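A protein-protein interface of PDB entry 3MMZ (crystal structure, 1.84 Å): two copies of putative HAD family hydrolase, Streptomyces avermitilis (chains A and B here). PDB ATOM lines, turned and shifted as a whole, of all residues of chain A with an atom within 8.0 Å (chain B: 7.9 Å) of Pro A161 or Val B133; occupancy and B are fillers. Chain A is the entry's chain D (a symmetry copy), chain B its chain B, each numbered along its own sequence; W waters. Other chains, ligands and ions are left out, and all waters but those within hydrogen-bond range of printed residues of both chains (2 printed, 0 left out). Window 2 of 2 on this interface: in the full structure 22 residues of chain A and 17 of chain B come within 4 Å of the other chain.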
ATOM      1  N   ARG A 152     -31.358  27.954  -1.810  1.00  0.00           N
ATOM      2  CA  ARG A 152     -29.924  28.036  -2.045  1.00  0.00           C
ATOM      3  C   ARG A 152     -29.128  27.581  -0.821  1.00  0.00           C
ATOM      4  O   ARG A 152     -28.140  26.868  -0.960  1.00  0.00           O
ATOM      5  CB  ARG A 152     -29.478  29.429  -2.479  1.00  0.00           C
ATOM      6  CG  ARG A 152     -28.105  29.373  -3.166  1.00  0.00           C
ATOM      7  CD  ARG A 152     -27.303  30.580  -2.881  1.00  0.00           C
ATOM      8  NE  ARG A 152     -25.891  30.457  -3.298  1.00  0.00           N
ATOM      9  CZ  ARG A 152     -24.943  29.842  -2.590  1.00  0.00           C
ATOM     10  NH1 ARG A 152     -23.692  29.812  -3.028  1.00  0.00           N
ATOM     11  NH2 ARG A 152     -25.243  29.240  -1.438  1.00  0.00           N
ATOM     12  N   ALA A 155     -29.334  23.860  -0.652  1.00  0.00           N
ATOM     13  CA  ALA A 155     -28.464  23.310  -1.685  1.00  0.00           C
ATOM     14  C   ALA A 155     -27.018  23.229  -1.185  1.00  0.00           C
ATOM     15  O   ALA A 155     -26.308  22.276  -1.503  1.00  0.00           O
ATOM     16  CB  ALA A 155     -28.562  24.136  -2.984  1.00  0.00           C
ATOM     17  N   SER A 156     -26.599  24.211  -0.379  1.00  0.00           N
ATOM     18  CA  SER A 156     -25.224  24.237   0.150  1.00  0.00           C
ATOM     19  C   SER A 156     -25.002  23.199   1.241  1.00  0.00           C
ATOM     20  O   SER A 156     -23.886  22.702   1.391  1.00  0.00           O
ATOM     21  CB  SER A 156     -24.793  25.637   0.629  1.00  0.00           C
ATOM     22  OG  SER A 156     -25.362  25.968   1.887  1.00  0.00           O
ATOM     23  N   TRP A 157     -26.055  22.855   1.988  1.00  0.00           N
ATOM     24  CA  TRP A 157     -25.971  21.730   2.930  1.00  0.00           C
ATOM     25  C   TRP A 157     -25.672  20.432   2.179  1.00  0.00           C
ATOM     26  O   TRP A 157     -24.817  19.644   2.584  1.00  0.00           O
ATOM     27  CB  TRP A 157     -27.288  21.543   3.694  1.00  0.00           C
ATOM     28  CG  TRP A 157     -27.690  22.667   4.581  1.00  0.00           C
ATOM     29  CD1 TRP A 157     -26.913  23.709   5.019  1.00  0.00           C
ATOM     30  CD2 TRP A 157     -28.971  22.838   5.189  1.00  0.00           C
ATOM     31  NE1 TRP A 157     -27.650  24.532   5.843  1.00  0.00           N
ATOM     32  CE2 TRP A 157     -28.917  24.023   5.957  1.00  0.00           C
ATOM     33  CE3 TRP A 157     -30.176  22.114   5.133  1.00  0.00           C
ATOM     34  CZ2 TRP A 157     -30.018  24.497   6.690  1.00  0.00           C
ATOM     35  CZ3 TRP A 157     -31.272  22.591   5.851  1.00  0.00           C
ATOM     36  CH2 TRP A 157     -31.179  23.765   6.626  1.00  0.00           C
ATOM     37  N   ILE A 158     -26.400  20.212   1.091  1.00  0.00           N
ATOM     38  CA  ILE A 158     -26.313  18.973   0.329  1.00  0.00           C
ATOM     39  C   ILE A 158     -25.030  18.917  -0.507  1.00  0.00           C
ATOM     40  O   ILE A 158     -24.364  17.878  -0.564  1.00  0.00           O
ATOM     41  CB  ILE A 158     -27.572  18.783  -0.590  1.00  0.00           C
ATOM     42  CG1 ILE A 158     -28.884  18.889   0.212  1.00  0.00           C
ATOM     43  CG2 ILE A 158     -27.498  17.469  -1.389  1.00  0.00           C
ATOM     44  CD1 ILE A 158     -28.990  17.914   1.367  1.00  0.00           C
ATOM     45  N   LEU A 159     -24.677  20.029  -1.145  1.00  0.00           N
ATOM     46  CA  LEU A 159     -23.601  20.025  -2.155  1.00  0.00           C
ATOM     47  C   LEU A 159     -22.306  20.720  -1.726  1.00  0.00           C
ATOM     48  O   LEU A 159     -21.284  20.631  -2.416  1.00  0.00           O
ATOM     49  CB  LEU A 159     -24.107  20.639  -3.465  1.00  0.00           C
ATOM     50  CG  LEU A 159     -25.330  19.959  -4.083  1.00  0.00           C
ATOM     51  CD1 LEU A 159     -25.888  20.819  -5.222  1.00  0.00           C
ATOM     52  CD2 LEU A 159     -25.016  18.536  -4.556  1.00  0.00           C
ATOM     53  N   GLY A 160     -22.348  21.399  -0.590  1.00  0.00           N
ATOM     54  CA  GLY A 160     -21.200  22.170  -0.124  1.00  0.00           C
ATOM     55  C   GLY A 160     -21.233  23.609  -0.609  1.00  0.00           C
ATOM     56  O   GLY A 160     -22.080  23.986  -1.431  1.00  0.00           O
ATOM     57  N   PRO A 161     -20.294  24.427  -0.108  1.00  0.00           N
ATOM     58  CA  PRO A 161     -20.288  25.867  -0.370  1.00  0.00           C
ATOM     59  C   PRO A 161     -20.174  26.251  -1.850  1.00  0.00           C
ATOM     60  O   PRO A 161     -20.658  27.316  -2.222  1.00  0.00           O
ATOM     61  CB  PRO A 161     -19.073  26.367   0.431  1.00  0.00           C
ATOM     62  CG  PRO A 161     -18.842  25.330   1.477  1.00  0.00           C
ATOM     63  CD  PRO A 161     -19.211  24.029   0.812  1.00  0.00           C
ATOM     64  N   SER A 162     -19.567  25.415  -2.697  1.00  0.00           N
ATOM     65  CA  SER A 162     -19.494  25.770  -4.127  1.00  0.00           C
ATOM     66  C   SER A 162     -20.628  25.183  -4.980  1.00  0.00           C
ATOM     67  O   SER A 162     -20.648  25.350  -6.215  1.00  0.00           O
ATOM     68  CB  SER A 162     -18.109  25.462  -4.724  1.00  0.00           C
ATOM     69  OG  SER A 162     -18.074  24.193  -5.359  1.00  0.00           O
ATOM     70  N   LEU A 163     -21.580  24.522  -4.310  1.00  0.00           N
ATOM     71  CA  LEU A 163     -22.720  23.869  -4.971  1.00  0.00           C
ATOM     72  C   LEU A 163     -22.250  22.799  -5.951  1.00  0.00           C
ATOM     73  O   LEU A 163     -22.928  22.488  -6.936  1.00  0.00           O
ATOM     74  CB  LEU A 163     -23.643  24.894  -5.655  1.00  0.00           C
ATOM     75  CG  LEU A 163     -24.179  26.030  -4.770  1.00  0.00           C
ATOM     76  CD1 LEU A 163     -25.150  26.911  -5.533  1.00  0.00           C
ATOM     77  CD2 LEU A 163     -24.834  25.505  -3.499  1.00  0.00           C
ATOM     78  N   ASP A 164     -21.075  22.247  -5.661  1.00  0.00           N
ATOM     79  CA  ASP A 164     -20.448  21.208  -6.472  1.00  0.00           C
ATOM     80  C   ASP A 164     -20.101  21.663  -7.902  1.00  0.00           C
ATOM     81  O   ASP A 164     -19.918  20.833  -8.799  1.00  0.00           O
ATOM     82  CB  ASP A 164     -21.315  19.937  -6.477  1.00  0.00           C
ATOM     83  CG  ASP A 164     -20.493  18.674  -6.607  1.00  0.00           C
ATOM     84  OD1 ASP A 164     -19.376  18.616  -6.048  1.00  0.00           O
ATOM     85  OD2 ASP A 164     -20.967  17.730  -7.268  1.00  0.00           O
ATOM     86  N   SER A 165     -20.004  22.981  -8.100  1.00  0.00           N
ATOM     87  CA  SER A 165     -19.614  23.568  -9.387  1.00  0.00           C
ATOM     88  C   SER A 165     -18.093  23.584  -9.539  1.00  0.00           C
ATOM     89  O   SER A 165     -17.564  23.628 -10.656  1.00  0.00           O
ATOM     90  CB  SER A 165     -20.148  24.999  -9.497  1.00  0.00           C
ATOM     91  OG  SER A 165     -19.492  25.850  -8.566  1.00  0.00           O
ATOM     92  N   LEU A 166     -17.405  23.568  -8.400  1.00  0.00           N
ATOM     93  CA  LEU A 166     -15.946  23.563  -8.351  1.00  0.00           C
ATOM     94  C   LEU A 166     -15.459  22.522  -7.359  1.00  0.00           C
ATOM     95  O   LEU A 166     -16.095  22.302  -6.324  1.00  0.00           O
ATOM     96  CB  LEU A 166     -15.417  24.929  -7.903  1.00  0.00           C
ATOM     97  CG  LEU A 166     -15.689  26.203  -8.698  1.00  0.00           C
ATOM     98  CD1 LEU A 166     -15.218  27.363  -7.863  1.00  0.00           C
ATOM     99  CD2 LEU A 166     -14.975  26.197 -10.043  1.00  0.00           C
ATOM    100  N   ASN B 110     -21.273  37.900  -7.319  1.00  0.00           N
ATOM    101  CA  ASN B 110     -21.929  37.622  -6.022  1.00  0.00           C
ATOM    102  C   ASN B 110     -22.134  36.162  -5.664  1.00  0.00           C
ATOM    103  O   ASN B 110     -22.433  35.869  -4.512  1.00  0.00           O
ATOM    104  CB  ASN B 110     -23.306  38.301  -5.945  1.00  0.00           C
ATOM    105  CG  ASN B 110     -24.367  37.541  -6.709  1.00  0.00           C
ATOM    106  OD1 ASN B 110     -24.273  37.395  -7.918  1.00  0.00           O
ATOM    107  ND2 ASN B 110     -25.385  37.062  -6.007  1.00  0.00           N
ATOM    108  N   ASP B 111     -22.045  35.259  -6.639  1.00  0.00           N
ATOM    109  CA  ASP B 111     -22.352  33.839  -6.363  1.00  0.00           C
ATOM    110  C   ASP B 111     -21.332  32.889  -7.003  1.00  0.00           C
ATOM    111  O   ASP B 111     -20.408  33.325  -7.702  1.00  0.00           O
ATOM    112  CB  ASP B 111     -23.801  33.476  -6.767  1.00  0.00           C
ATOM    113  CG  ASP B 111     -24.432  32.376  -5.858  1.00  0.00           C
ATOM    114  OD1 ASP B 111     -23.712  31.606  -5.190  1.00  0.00           O
ATOM    115  OD2 ASP B 111     -25.676  32.272  -5.809  1.00  0.00           O
ATOM    116  N   VAL B 112     -21.503  31.593  -6.756  1.00  0.00           N
ATOM    117  CA  VAL B 112     -20.472  30.601  -7.079  1.00  0.00           C
ATOM    118  C   VAL B 112     -20.192  30.448  -8.577  1.00  0.00           C
ATOM    119  O   VAL B 112     -19.095  30.049  -8.951  1.00  0.00           O
ATOM    120  CB  VAL B 112     -20.726  29.226  -6.390  1.00  0.00           C
ATOM    121  CG1 VAL B 112     -20.733  29.395  -4.879  1.00  0.00           C
ATOM    122  CG2 VAL B 112     -22.029  28.576  -6.886  1.00  0.00           C
ATOM    123  N   LEU B 115     -17.127  32.424  -9.591  1.00  0.00           N
ATOM    124  CA  LEU B 115     -15.779  32.046  -9.150  1.00  0.00           C
ATOM    125  C   LEU B 115     -14.807  31.733 -10.303  1.00  0.00           C
ATOM    126  O   LEU B 115     -13.668  32.178 -10.260  1.00  0.00           O
ATOM    127  CB  LEU B 115     -15.814  30.903  -8.126  1.00  0.00           C
ATOM    128  CG  LEU B 115     -16.456  31.254  -6.779  1.00  0.00           C
ATOM    129  CD1 LEU B 115     -16.725  29.984  -5.961  1.00  0.00           C
ATOM    130  CD2 LEU B 115     -15.607  32.265  -5.989  1.00  0.00           C
ATOM    131  N   PHE B 118     -13.690  35.040 -11.545  1.00  0.00           N
ATOM    132  CA  PHE B 118     -12.769  35.605 -10.555  1.00  0.00           C
ATOM    133  C   PHE B 118     -11.331  35.118 -10.780  1.00  0.00           C
ATOM    134  O   PHE B 118     -10.376  35.901 -10.677  1.00  0.00           O
ATOM    135  CB  PHE B 118     -13.201  35.190  -9.135  1.00  0.00           C
ATOM    136  CG  PHE B 118     -14.226  36.099  -8.489  1.00  0.00           C
ATOM    137  CD1 PHE B 118     -15.012  36.984  -9.242  1.00  0.00           C
ATOM    138  CD2 PHE B 118     -14.403  36.059  -7.101  1.00  0.00           C
ATOM    139  CE1 PHE B 118     -15.954  37.813  -8.619  1.00  0.00           C
ATOM    140  CE2 PHE B 118     -15.346  36.871  -6.461  1.00  0.00           C
ATOM    141  CZ  PHE B 118     -16.129  37.757  -7.213  1.00  0.00           C
ATOM    142  N   ALA B 126     -16.185  41.297  -5.022  1.00  0.00           N
ATOM    143  CA  ALA B 126     -17.481  40.785  -4.574  1.00  0.00           C
ATOM    144  C   ALA B 126     -18.312  41.914  -3.963  1.00  0.00           C
ATOM    145  O   ALA B 126     -17.783  42.780  -3.251  1.00  0.00           O
ATOM    146  CB  ALA B 126     -17.307  39.635  -3.554  1.00  0.00           C
ATOM    147  N   ALA B 130     -22.489  39.085  -1.245  1.00  0.00           N
ATOM    148  CA  ALA B 130     -22.010  37.878  -1.908  1.00  0.00           C
ATOM    149  C   ALA B 130     -21.979  36.706  -0.945  1.00  0.00           C
ATOM    150  O   ALA B 130     -21.833  36.892   0.270  1.00  0.00           O
ATOM    151  CB  ALA B 130     -20.597  38.110  -2.502  1.00  0.00           C
ATOM    152  N   HIS B 131     -22.099  35.495  -1.492  1.00  0.00           N
ATOM    153  CA  HIS B 131     -22.052  34.296  -0.675  1.00  0.00           C
ATOM    154  C   HIS B 131     -20.656  34.061  -0.133  1.00  0.00           C
ATOM    155  O   HIS B 131     -19.674  34.530  -0.715  1.00  0.00           O
ATOM    156  CB  HIS B 131     -22.612  33.095  -1.444  1.00  0.00           C
ATOM    157  CG  HIS B 131     -24.080  33.219  -1.695  1.00  0.00           C
ATOM    158  ND1 HIS B 131     -25.025  32.839  -0.765  1.00  0.00           N
ATOM    159  CD2 HIS B 131     -24.763  33.761  -2.728  1.00  0.00           C
ATOM    160  CE1 HIS B 131     -26.231  33.126  -1.225  1.00  0.00           C
ATOM    161  NE2 HIS B 131     -26.101  33.682  -2.418  1.00  0.00           N
ATOM    162  N   ASP B 132     -20.590  33.378   1.009  1.00  0.00           N
ATOM    163  CA  ASP B 132     -19.333  33.178   1.763  1.00  0.00           C
ATOM    164  C   ASP B 132     -18.053  33.039   0.934  1.00  0.00           C
ATOM    165  O   ASP B 132     -17.137  33.876   1.046  1.00  0.00           O
ATOM    166  CB  ASP B 132     -19.460  31.999   2.740  1.00  0.00           C
ATOM    167  CG  ASP B 132     -20.115  30.767   2.111  1.00  0.00           C
ATOM    168  OD1 ASP B 132     -20.146  30.635   0.866  1.00  0.00           O
ATOM    169  OD2 ASP B 132     -20.607  29.917   2.885  1.00  0.00           O
ATOM    170  N   VAL B 133     -17.978  31.993   0.111  1.00  0.00           N
ATOM    171  CA  VAL B 133     -16.735  31.668  -0.599  1.00  0.00           C
ATOM    172  C   VAL B 133     -16.384  32.714  -1.653  1.00  0.00           C
ATOM    173  O   VAL B 133     -15.217  32.885  -2.013  1.00  0.00           O
ATOM    174  CB  VAL B 133     -16.767  30.246  -1.231  1.00  0.00           C
ATOM    175  CG1 VAL B 133     -16.840  29.183  -0.147  1.00  0.00           C
ATOM    176  CG2 VAL B 133     -17.939  30.093  -2.190  1.00  0.00           C
ATOM    177  N   VAL B 134     -17.406  33.406  -2.137  1.00  0.00           N
ATOM    178  CA  VAL B 134     -17.234  34.472  -3.126  1.00  0.00           C
ATOM    179  C   VAL B 134     -16.629  35.713  -2.480  1.00  0.00           C
ATOM    180  O   VAL B 134     -15.711  36.315  -3.038  1.00  0.00           O
ATOM    181  CB  VAL B 134     -18.577  34.813  -3.817  1.00  0.00           C
ATOM    182  CG1 VAL B 134     -18.389  35.915  -4.890  1.00  0.00           C
ATOM    183  CG2 VAL B 134     -19.146  33.551  -4.438  1.00  0.00           C
ATOM    184  N   ARG B 135     -17.144  36.094  -1.309  1.00  0.00           N
ATOM    185  CA  ARG B 135     -16.562  37.209  -0.544  1.00  0.00           C
ATOM    186  C   ARG B 135     -15.065  36.993  -0.318  1.00  0.00           C
ATOM    187  O   ARG B 135     -14.265  37.904  -0.527  1.00  0.00           O
ATOM    188  CB  ARG B 135     -17.259  37.360   0.824  1.00  0.00           C
ATOM    189  CG  ARG B 135     -18.216  38.535   0.968  1.00  0.00           C
ATOM    190  CD  ARG B 135     -18.757  38.664   2.419  1.00  0.00           C
ATOM    191  NE  ARG B 135     -19.926  37.815   2.594  1.00  0.00           N
ATOM    192  CZ  ARG B 135     -19.902  36.591   3.118  1.00  0.00           C
ATOM    193  NH1 ARG B 135     -18.757  36.058   3.577  1.00  0.00           N
ATOM    194  NH2 ARG B 135     -21.031  35.901   3.202  1.00  0.00           N
ATOM    195  N   GLY B 136     -14.695  35.783   0.099  1.00  0.00           N
ATOM    196  CA  GLY B 136     -13.289  35.439   0.335  1.00  0.00           C
ATOM    197  C   GLY B 136     -12.429  35.465  -0.921  1.00  0.00           C
ATOM    198  O   GLY B 136     -11.304  35.956  -0.901  1.00  0.00           O
ATOM    199  N   ALA B 137     -12.950  34.921  -2.018  1.00  0.00           N
ATOM    200  CA  ALA B 137     -12.162  34.796  -3.254  1.00  0.00           C
ATOM    201  C   ALA B 137     -11.896  36.133  -3.950  1.00  0.00           C
ATOM    202  O   ALA B 137     -10.951  36.250  -4.727  1.00  0.00           O
ATOM    203  CB  ALA B 137     -12.820  33.805  -4.210  1.00  0.00           C
ATOM    204  N   ALA B 138     -12.715  37.140  -3.657  1.00  0.00           N
ATOM    205  CA  ALA B 138     -12.530  38.476  -4.216  1.00  0.00           C
ATOM    206  C   ALA B 138     -11.228  39.111  -3.724  1.00  0.00           C
ATOM    207  O   ALA B 138     -10.761  38.805  -2.624  1.00  0.00           O
ATOM    208  CB  ALA B 138     -13.701  39.365  -3.837  1.00  0.00           C
HETATM  209  O   HOH W   1     -18.353  27.840  -9.947  1.00  0.00           O
HETATM  210  O   HOH W   2     -21.722  29.389  -1.110  1.00  0.00           O
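Water W1 bridges O of Val B112 (2.5 Å) and OG of Ser A165 (2.7 Å). Water W2 lies within hydrogen-bond range of the backbone carbonyl oxygen (O) of Pro A161 (2.6 Å), the guanidinium group (NH1) of Arg A152 (2.8 Å) and the side-chain carboxylate (OD1) of Asp B132 (2.8 Å).
Of the 15 printed residues of chain B, 5 touch a printed residue of chain A. Hydrophobic or aromatic side chains of chain B within 4 Å of the printed part of chain A: Val B112, Leu B115, His B131 and Val B133. Among the printed residues, 8 pairs touch across the chains. Among the printed residues, Asp or Glu carboxylates within 4 Å of a Lys or Arg side-chain nitrogen of the other chain: Arg A152 with Asp B111 (2.8 Å).
Among the printed residues, merely in contact across the chains: Pro A161 with Val B112, Arg A152 with Val B112, Leu A166 with Leu B115, Ser A162 with Val B112, Pro A161 with Val B133 and Leu A163 with Val B112.
The side-chain carboxylate of Asp B111 lies within salt-bridge range of the guanidinium group of Arg A152, at 2.8 Å. The guanidinium group of Arg A152 is in hydrogen-bond range of a ring nitrogen (NE2) of His B131, 3.3 Å away.
OG of Ser A162 is in hydrogen-bond range of O of Leu A166, 2.9 Å away. The backbone carbonyl oxygen (O) of Ser A162 is in hydrogen-bond range of the side-chain hydroxyl (OG) of Ser A165. N of His B131 sits at hydrogen-bond distance from O of Asn B110 (3.1 Å).
No position is printed for both chains. Of the 8 pairs that touch across the chains among the printed residues, none has its exchanged pair printed and touching as well.
Of the printed residues of chain A, Val B133 touches Pro A161. No residue of chain B comes within 4 Å of Gly A160. Printed residues of chain B within 4 Å of Leu A166: Leu B115. Of the printed residues of chain B, Ser A162 touches Val B112. Printed residues of chain A within 4 Å of Asp B111: Arg A152 (2.8 Å). Of the printed residues of chain A, Val B112 touches Arg A152, Pro A161, Ser A162 and Leu A163. Of the printed residues of chain B, Leu A163 touches Val B112 (3.8 Å). Leu A159 touches none of the printed residues of chain B. The nearest residue of chain A that does not touch Val B133 is Ser A162 (5.0 Å). The nearest printed residue of chain A that does not touch Asp B111 is Leu A163 (4.9 Å).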
